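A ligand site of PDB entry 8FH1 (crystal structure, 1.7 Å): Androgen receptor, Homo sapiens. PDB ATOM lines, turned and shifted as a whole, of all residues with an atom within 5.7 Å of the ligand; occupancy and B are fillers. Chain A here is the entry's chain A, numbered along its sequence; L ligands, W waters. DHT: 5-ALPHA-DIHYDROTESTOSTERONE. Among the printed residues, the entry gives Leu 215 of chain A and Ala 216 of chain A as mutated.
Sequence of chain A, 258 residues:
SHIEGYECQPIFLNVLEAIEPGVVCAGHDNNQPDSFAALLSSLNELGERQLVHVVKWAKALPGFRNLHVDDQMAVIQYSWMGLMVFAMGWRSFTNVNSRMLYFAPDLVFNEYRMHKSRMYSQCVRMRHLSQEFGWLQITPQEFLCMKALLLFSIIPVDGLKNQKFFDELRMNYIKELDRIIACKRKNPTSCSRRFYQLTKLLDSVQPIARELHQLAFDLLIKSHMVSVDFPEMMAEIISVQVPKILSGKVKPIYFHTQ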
ATOM      1  N   LEU A  40      30.892  24.294   9.302  1.00  0.00           N
ATOM      2  CA  LEU A  40      29.526  24.220   8.806  1.00  0.00           C
ATOM      3  C   LEU A  40      28.593  25.096   9.634  1.00  0.00           C
ATOM      4  O   LEU A  40      27.677  25.695   9.080  1.00  0.00           O
ATOM      5  CB  LEU A  40      29.015  22.776   8.733  1.00  0.00           C
ATOM      6  CG  LEU A  40      29.213  22.143   7.349  1.00  0.00           C
ATOM      7  CD1 LEU A  40      28.398  22.857   6.233  1.00  0.00           C
ATOM      8  CD2 LEU A  40      30.704  22.006   6.961  1.00  0.00           C
ATOM      9  N   LEU A  43      29.028  28.528   8.208  1.00  0.00           N
ATOM     10  CA  LEU A  43      28.389  28.635   6.898  1.00  0.00           C
ATOM     11  C   LEU A  43      26.880  28.800   7.056  1.00  0.00           C
ATOM     12  O   LEU A  43      26.278  29.640   6.376  1.00  0.00           O
ATOM     13  CB  LEU A  43      28.696  27.410   6.021  1.00  0.00           C
ATOM     14  CG  LEU A  43      30.118  27.397   5.400  1.00  0.00           C
ATOM     15  CD1 LEU A  43      30.410  26.037   4.760  1.00  0.00           C
ATOM     16  CD2 LEU A  43      30.272  28.516   4.366  1.00  0.00           C
ATOM     17  N   ASN A  44      26.281  28.059   7.997  1.00  0.00           N
ATOM     18  CA  ASN A  44      24.837  28.191   8.219  1.00  0.00           C
ATOM     19  C   ASN A  44      24.485  29.566   8.752  1.00  0.00           C
ATOM     20  O   ASN A  44      23.443  30.127   8.426  1.00  0.00           O
ATOM     21  CB  ASN A  44      24.342  27.130   9.210  1.00  0.00           C
ATOM     22  CG  ASN A  44      24.342  25.733   8.629  1.00  0.00           C
ATOM     23  OD1 ASN A  44      24.332  25.561   7.412  1.00  0.00           O
ATOM     24  ND2 ASN A  44      24.367  24.723   9.494  1.00  0.00           N
ATOM     25  N   LEU A  46      26.237  32.316   8.186  1.00  0.00           N
ATOM     26  CA  LEU A  46      26.378  33.212   7.034  1.00  0.00           C
ATOM     27  C   LEU A  46      25.150  33.137   6.137  1.00  0.00           C
ATOM     28  O   LEU A  46      24.657  34.171   5.667  1.00  0.00           O
ATOM     29  CB  LEU A  46      27.620  32.841   6.224  1.00  0.00           C
ATOM     30  CG  LEU A  46      27.893  33.714   5.002  1.00  0.00           C
ATOM     31  CD1 LEU A  46      28.156  35.173   5.500  1.00  0.00           C
ATOM     32  CD2 LEU A  46      29.141  33.191   4.339  1.00  0.00           C
ATOM     33  N   GLY A  47      24.669  31.925   5.846  1.00  0.00           N
ATOM     34  CA  GLY A  47      23.445  31.801   5.063  1.00  0.00           C
ATOM     35  C   GLY A  47      22.281  32.558   5.678  1.00  0.00           C
ATOM     36  O   GLY A  47      21.526  33.227   4.980  1.00  0.00           O
ATOM     37  N   GLN A  50      22.918  36.290   5.140  1.00  0.00           N
ATOM     38  CA  GLN A  50      22.773  36.703   3.748  1.00  0.00           C
ATOM     39  C   GLN A  50      21.309  36.667   3.327  1.00  0.00           C
ATOM     40  O   GLN A  50      20.870  37.523   2.549  1.00  0.00           O
ATOM     41  CB  GLN A  50      23.621  35.804   2.835  1.00  0.00           C
ATOM     42  CG  GLN A  50      25.093  36.283   2.783  1.00  0.00           C
ATOM     43  CD  GLN A  50      25.956  35.506   1.833  1.00  0.00           C
ATOM     44  OE1 GLN A  50      25.443  34.779   0.982  1.00  0.00           O
ATOM     45  NE2 GLN A  50      27.276  35.617   1.996  1.00  0.00           N
ATOM     46  N   TRP A  80      17.494  31.123  -3.550  1.00  0.00           N
ATOM     47  CA  TRP A  80      18.522  31.712  -2.694  1.00  0.00           C
ATOM     48  C   TRP A  80      19.868  31.011  -2.832  1.00  0.00           C
ATOM     49  O   TRP A  80      20.909  31.676  -2.859  1.00  0.00           O
ATOM     50  CB  TRP A  80      18.065  31.727  -1.237  1.00  0.00           C
ATOM     51  CG  TRP A  80      17.854  30.362  -0.654  1.00  0.00           C
ATOM     52  CD1 TRP A  80      16.723  29.606  -0.749  1.00  0.00           C
ATOM     53  CD2 TRP A  80      18.786  29.585   0.108  1.00  0.00           C
ATOM     54  NE1 TRP A  80      16.888  28.420  -0.094  1.00  0.00           N
ATOM     55  CE2 TRP A  80      18.145  28.383   0.450  1.00  0.00           C
ATOM     56  CE3 TRP A  80      20.089  29.812   0.552  1.00  0.00           C
ATOM     57  CZ2 TRP A  80      18.770  27.395   1.195  1.00  0.00           C
ATOM     58  CZ3 TRP A  80      20.708  28.843   1.316  1.00  0.00           C
ATOM     59  CH2 TRP A  80      20.048  27.635   1.627  1.00  0.00           C
ATOM     60  N   MET A  81      19.889  29.666  -2.858  1.00  0.00           N
ATOM     61  CA  MET A  81      21.161  28.957  -3.032  1.00  0.00           C
ATOM     62  C   MET A  81      21.934  29.440  -4.234  1.00  0.00           C
ATOM     63  O   MET A  81      23.147  29.712  -4.145  1.00  0.00           O
ATOM     64  CB  MET A  81      20.933  27.455  -3.246  1.00  0.00           C
ATOM     65  CG  MET A  81      22.142  26.583  -2.973  1.00  0.00           C
ATOM     66  SD  MET A  81      23.098  26.744  -1.464  1.00  0.00           S
ATOM     67  CE  MET A  81      22.126  25.587  -0.538  1.00  0.00           C
ATOM     68  N   MET A  84      23.211  32.984  -3.929  1.00  0.00           N
ATOM     69  CA  MET A  84      24.296  33.165  -2.979  1.00  0.00           C
ATOM     70  C   MET A  84      25.589  32.557  -3.510  1.00  0.00           C
ATOM     71  O   MET A  84      26.679  33.077  -3.269  1.00  0.00           O
ATOM     72  CB  MET A  84      23.899  32.474  -1.673  1.00  0.00           C
ATOM     73  CG  MET A  84      23.072  33.331  -0.772  1.00  0.00           C
ATOM     74  SD  MET A  84      22.652  32.527   0.779  1.00  0.00           S
ATOM     75  CE  MET A  84      21.192  33.494   1.240  1.00  0.00           C
ATOM     76  N   VAL A  85      25.495  31.468  -4.280  1.00  0.00           N
ATOM     77  CA  VAL A  85      26.720  30.857  -4.788  1.00  0.00           C
ATOM     78  C   VAL A  85      27.312  31.712  -5.910  1.00  0.00           C
ATOM     79  O   VAL A  85      28.529  31.923  -5.986  1.00  0.00           O
ATOM     80  CB  VAL A  85      26.456  29.429  -5.297  1.00  0.00           C
ATOM     81  CG1 VAL A  85      27.621  28.949  -6.145  1.00  0.00           C
ATOM     82  CG2 VAL A  85      26.210  28.454  -4.118  1.00  0.00           C
ATOM     83  N   MET A  88      28.996  34.643  -4.308  1.00  0.00           N
ATOM     84  CA  MET A  88      30.251  34.229  -3.700  1.00  0.00           C
ATOM     85  C   MET A  88      31.323  33.966  -4.748  1.00  0.00           C
ATOM     86  O   MET A  88      32.505  34.294  -4.529  1.00  0.00           O
ATOM     87  CB  MET A  88      29.969  33.005  -2.806  1.00  0.00           C
ATOM     88  CG  MET A  88      31.100  32.440  -1.970  1.00  0.00           C
ATOM     89  SD  MET A  88      32.326  31.536  -2.945  1.00  0.00           S
ATOM     90  CE  MET A  88      31.294  30.099  -3.193  1.00  0.00           C
ATOM     91  N   ARG A  91      32.709  37.378  -5.590  1.00  0.00           N
ATOM     92  CA  ARG A  91      33.573  37.821  -4.492  1.00  0.00           C
ATOM     93  C   ARG A  91      34.921  37.124  -4.540  1.00  0.00           C
ATOM     94  O   ARG A  91      35.972  37.730  -4.306  1.00  0.00           O
ATOM     95  CB  ARG A  91      32.904  37.497  -3.150  1.00  0.00           C
ATOM     96  CG  ARG A  91      31.800  38.403  -2.772  1.00  0.00           C
ATOM     97  CD  ARG A  91      31.540  38.299  -1.276  1.00  0.00           C
ATOM     98  NE  ARG A  91      31.086  36.984  -0.821  1.00  0.00           N
ATOM     99  CZ  ARG A  91      29.857  36.498  -0.996  1.00  0.00           C
ATOM    100  NH1 ARG A  91      28.924  37.149  -1.681  1.00  0.00           N
ATOM    101  NH2 ARG A  91      29.550  35.339  -0.425  1.00  0.00           N
ATOM    102  N   TYR A 102      35.908  32.791  -1.115  1.00  0.00           N
ATOM    103  CA  TYR A 102      35.688  33.946  -0.252  1.00  0.00           C
ATOM    104  C   TYR A 102      34.223  34.006   0.194  1.00  0.00           C
ATOM    105  O   TYR A 102      33.439  34.834  -0.252  1.00  0.00           O
ATOM    106  CB  TYR A 102      36.075  35.227  -0.995  1.00  0.00           C
ATOM    107  CG  TYR A 102      36.271  36.471  -0.152  1.00  0.00           C
ATOM    108  CD1 TYR A 102      35.213  37.327   0.137  1.00  0.00           C
ATOM    109  CD2 TYR A 102      37.524  36.790   0.357  1.00  0.00           C
ATOM    110  CE1 TYR A 102      35.403  38.495   0.899  1.00  0.00           C
ATOM    111  CE2 TYR A 102      37.716  37.938   1.130  1.00  0.00           C
ATOM    112  CZ  TYR A 102      36.664  38.774   1.400  1.00  0.00           C
ATOM    113  OH  TYR A 102      36.895  39.907   2.159  1.00  0.00           O
ATOM    114  N   PHE A 103      33.836  33.059   1.071  1.00  0.00           N
ATOM    115  CA  PHE A 103      32.445  33.087   1.541  1.00  0.00           C
ATOM    116  C   PHE A 103      32.149  34.415   2.223  1.00  0.00           C
ATOM    117  O   PHE A 103      31.082  35.010   2.029  1.00  0.00           O
ATOM    118  CB  PHE A 103      32.180  31.918   2.487  1.00  0.00           C
ATOM    119  CG  PHE A 103      32.218  30.583   1.802  1.00  0.00           C
ATOM    120  CD1 PHE A 103      31.142  30.137   1.024  1.00  0.00           C
ATOM    121  CD2 PHE A 103      33.329  29.774   1.928  1.00  0.00           C
ATOM    122  CE1 PHE A 103      31.187  28.949   0.398  1.00  0.00           C
ATOM    123  CE2 PHE A 103      33.372  28.537   1.290  1.00  0.00           C
ATOM    124  CZ  PHE A 103      32.291  28.121   0.532  1.00  0.00           C
ATOM    125  N   MET A 119      33.242  19.211   2.161  1.00  0.00           N
ATOM    126  CA  MET A 119      32.655  19.712   0.922  1.00  0.00           C
ATOM    127  C   MET A 119      33.679  19.893  -0.181  1.00  0.00           C
ATOM    128  O   MET A 119      33.498  20.732  -1.057  1.00  0.00           O
ATOM    129  CB  MET A 119      31.900  21.038   1.137  1.00  0.00           C
ATOM    130  CG  MET A 119      30.999  21.095   2.367  1.00  0.00           C
ATOM    131  SD  MET A 119      30.561  22.787   2.859  1.00  0.00           S
ATOM    132  CE  MET A 119      30.591  23.575   1.252  1.00  0.00           C
ATOM    133  N   MET A 126      32.573  25.092  -7.197  1.00  0.00           N
ATOM    134  CA  MET A 126      32.304  26.503  -6.913  1.00  0.00           C
ATOM    135  C   MET A 126      33.508  27.334  -7.338  1.00  0.00           C
ATOM    136  O   MET A 126      33.380  28.438  -7.887  1.00  0.00           O
ATOM    137  CB  MET A 126      32.046  26.548  -5.393  1.00  0.00           C
ATOM    138  CG  MET A 126      30.558  26.549  -5.081  1.00  0.00           C
ATOM    139  SD  MET A 126      30.039  26.747  -3.365  1.00  0.00           S
ATOM    140  CE  MET A 126      30.878  25.383  -2.561  1.00  0.00           C
ATOM    141  N   LEU A 212      24.512  21.481  -3.513  1.00  0.00           N
ATOM    142  CA  LEU A 212      24.490  22.126  -2.211  1.00  0.00           C
ATOM    143  C   LEU A 212      23.129  21.976  -1.538  1.00  0.00           C
ATOM    144  O   LEU A 212      23.060  21.844  -0.305  1.00  0.00           O
ATOM    145  CB  LEU A 212      24.855  23.614  -2.353  1.00  0.00           C
ATOM    146  CG  LEU A 212      26.305  23.802  -2.849  1.00  0.00           C
ATOM    147  CD1 LEU A 212      26.494  25.220  -3.277  1.00  0.00           C
ATOM    148  CD2 LEU A 212      27.366  23.365  -1.824  1.00  0.00           C
ATOM    149  N   LEU A 215      23.387  18.557   0.013  1.00  0.00           N
ATOM    150  CA  LEU A 215      24.252  18.581   1.177  1.00  0.00           C
ATOM    151  C   LEU A 215      23.563  19.240   2.356  1.00  0.00           C
ATOM    152  O   LEU A 215      23.611  18.736   3.479  1.00  0.00           O
ATOM    153  CB  LEU A 215      25.550  19.315   0.830  1.00  0.00           C
ATOM    154  CG  LEU A 215      26.632  19.571   1.879  1.00  0.00           C
ATOM    155  CD1 LEU A 215      27.234  18.284   2.434  1.00  0.00           C
ATOM    156  CD2 LEU A 215      27.706  20.462   1.257  1.00  0.00           C
ATOM    157  N   ALA A 216      22.928  20.400   2.106  1.00  0.00           N
ATOM    158  CA  ALA A 216      22.217  21.120   3.164  1.00  0.00           C
ATOM    159  C   ALA A 216      21.166  20.234   3.808  1.00  0.00           C
ATOM    160  O   ALA A 216      21.041  20.190   5.047  1.00  0.00           O
ATOM    161  CB  ALA A 216      21.571  22.384   2.576  1.00  0.00           C
ATOM    162  N   LEU A 219      22.602  17.389   5.853  1.00  0.00           N
ATOM    163  CA  LEU A 219      23.228  17.854   7.081  1.00  0.00           C
ATOM    164  C   LEU A 219      22.175  18.307   8.105  1.00  0.00           C
ATOM    165  O   LEU A 219      22.354  18.075   9.303  1.00  0.00           O
ATOM    166  CB  LEU A 219      24.249  18.936   6.745  1.00  0.00           C
ATOM    167  CG  LEU A 219      24.989  19.520   7.939  1.00  0.00           C
ATOM    168  CD1 LEU A 219      25.921  18.455   8.466  1.00  0.00           C
ATOM    169  CD2 LEU A 219      25.800  20.700   7.446  1.00  0.00           C
ATOM    170  N   PHE A 230      21.797  24.830  13.116  1.00  0.00           N
ATOM    171  CA  PHE A 230      21.053  25.462  12.035  1.00  0.00           C
ATOM    172  C   PHE A 230      20.208  26.608  12.561  1.00  0.00           C
ATOM    173  O   PHE A 230      19.299  26.379  13.387  1.00  0.00           O
ATOM    174  CB  PHE A 230      20.163  24.454  11.289  1.00  0.00           C
ATOM    175  CG  PHE A 230      20.879  23.704  10.212  1.00  0.00           C
ATOM    176  CD1 PHE A 230      21.632  22.575  10.530  1.00  0.00           C
ATOM    177  CD2 PHE A 230      20.822  24.130   8.896  1.00  0.00           C
ATOM    178  CE1 PHE A 230      22.313  21.892   9.570  1.00  0.00           C
ATOM    179  CE2 PHE A 230      21.503  23.420   7.902  1.00  0.00           C
ATOM    180  CZ  PHE A 230      22.244  22.301   8.248  1.00  0.00           C
ATOM    181  N   MET A 234      17.140  29.150   8.200  1.00  0.00           N
ATOM    182  CA  MET A 234      17.790  28.095   7.435  1.00  0.00           C
ATOM    183  C   MET A 234      17.098  26.754   7.674  1.00  0.00           C
ATOM    184  O   MET A 234      16.855  25.999   6.720  1.00  0.00           O
ATOM    185  CB  MET A 234      19.277  28.012   7.767  1.00  0.00           C
ATOM    186  CG  MET A 234      20.126  29.209   7.248  1.00  0.00           C
ATOM    187  SD  MET A 234      20.317  29.272   5.440  1.00  0.00           S
ATOM    188  CE  MET A 234      21.755  28.253   5.191  1.00  0.00           C
ATOM    189  N   ILE A 238      15.266  24.816   4.624  1.00  0.00           N
ATOM    190  CA  ILE A 238      15.859  23.555   4.186  1.00  0.00           C
ATOM    191  C   ILE A 238      14.904  22.382   4.398  1.00  0.00           C
ATOM    192  O   ILE A 238      14.989  21.377   3.681  1.00  0.00           O
ATOM    193  CB  ILE A 238      17.216  23.324   4.877  1.00  0.00           C
ATOM    194  CG1 ILE A 238      18.230  24.367   4.383  1.00  0.00           C
ATOM    195  CG2 ILE A 238      17.739  21.965   4.528  1.00  0.00           C
ATOM    196  CD1 ILE A 238      19.494  24.439   5.252  1.00  0.00           C
HETATM  197  C1  DHT L   1      26.410  30.634   2.497  1.00  0.00           C
HETATM  198  C2  DHT L   1      26.585  31.927   1.685  1.00  0.00           C
HETATM  199  C3  DHT L   1      27.604  31.785   0.601  1.00  0.00           C
HETATM  200  O3  DHT L   1      28.428  32.643   0.369  1.00  0.00           O
HETATM  201  C4  DHT L   1      27.531  30.513  -0.205  1.00  0.00           C
HETATM  202  C5  DHT L   1      27.392  29.281   0.692  1.00  0.00           C
HETATM  203  C6  DHT L   1      27.269  28.008  -0.149  1.00  0.00           C
HETATM  204  C7  DHT L   1      27.206  26.775   0.751  1.00  0.00           C
HETATM  205  C8  DHT L   1      26.039  26.832   1.719  1.00  0.00           C
HETATM  206  C9  DHT L   1      26.128  28.121   2.543  1.00  0.00           C
HETATM  207  C10 DHT L   1      26.168  29.388   1.632  1.00  0.00           C
HETATM  208  C11 DHT L   1      25.017  28.187   3.583  1.00  0.00           C
HETATM  209  C12 DHT L   1      25.005  26.957   4.496  1.00  0.00           C
HETATM  210  C13 DHT L   1      24.950  25.653   3.689  1.00  0.00           C
HETATM  211  C14 DHT L   1      26.136  25.674   2.708  1.00  0.00           C
HETATM  212  C15 DHT L   1      26.115  24.249   2.139  1.00  0.00           C
HETATM  213  C16 DHT L   1      25.608  23.379   3.313  1.00  0.00           C
HETATM  214  C17 DHT L   1      25.306  24.365   4.448  1.00  0.00           C
HETATM  215  O17 DHT L   1      24.200  23.873   5.199  1.00  0.00           O
HETATM  216  C18 DHT L   1      23.589  25.501   2.995  1.00  0.00           C
HETATM  217  C19 DHT L   1      24.859  29.618   0.864  1.00  0.00           C
HETATM  218  O   HOH W   1      26.728  35.031  -1.261  1.00  0.00           O
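An oxygen (O17) of the ligand sits at hydrogen-bond distance from the side-chain amide oxygen of Asn 44.
NH2 of Arg 91 sits at hydrogen-bond distance from O3 of the ligand, at 3.0 Å.
The side-chain amide nitrogen (ND2) of Asn 44 sits close to the backbone carbonyl oxygen (O) of Leu 40 (3.5 Å).
The guanidinium group (NH2) of Arg 91 lies close to the side-chain amide nitrogen (NE2) of Gln 50.
The guanidinium group (NH2) of Arg 91 lies within hydrogen-bond range of the backbone carbonyl oxygen (O) of Phe 103 (2.9 Å).
The guanidinium group of Arg 91 is in hydrogen-bond range of the backbone carbonyl oxygen of Tyr 102, at 3.2 Å.
The side-chain amide oxygen (OE1) of Gln 50 sits close to the side-chain sulfur (SD) of Met 84 (3.6 Å).
Merely in contact with the ligand: Leu 40 (3.9 Å), Leu 43 (3.4 Å), Leu 46 (3.9 Å), Gly 47 (3.99 Å), Gln 50 (3.2 Å), Met 81 (3.8 Å), Met 84 (3.7 Å), Met 88 (3.5 Å), Phe 103 (3.8 Å), Ala 216 (3.7 Å), Phe 230 (3.8 Å) and Met 234 (3.6 Å).
The nearest printed residue that does not touch the ligand is Val 85 (4.1 Å).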
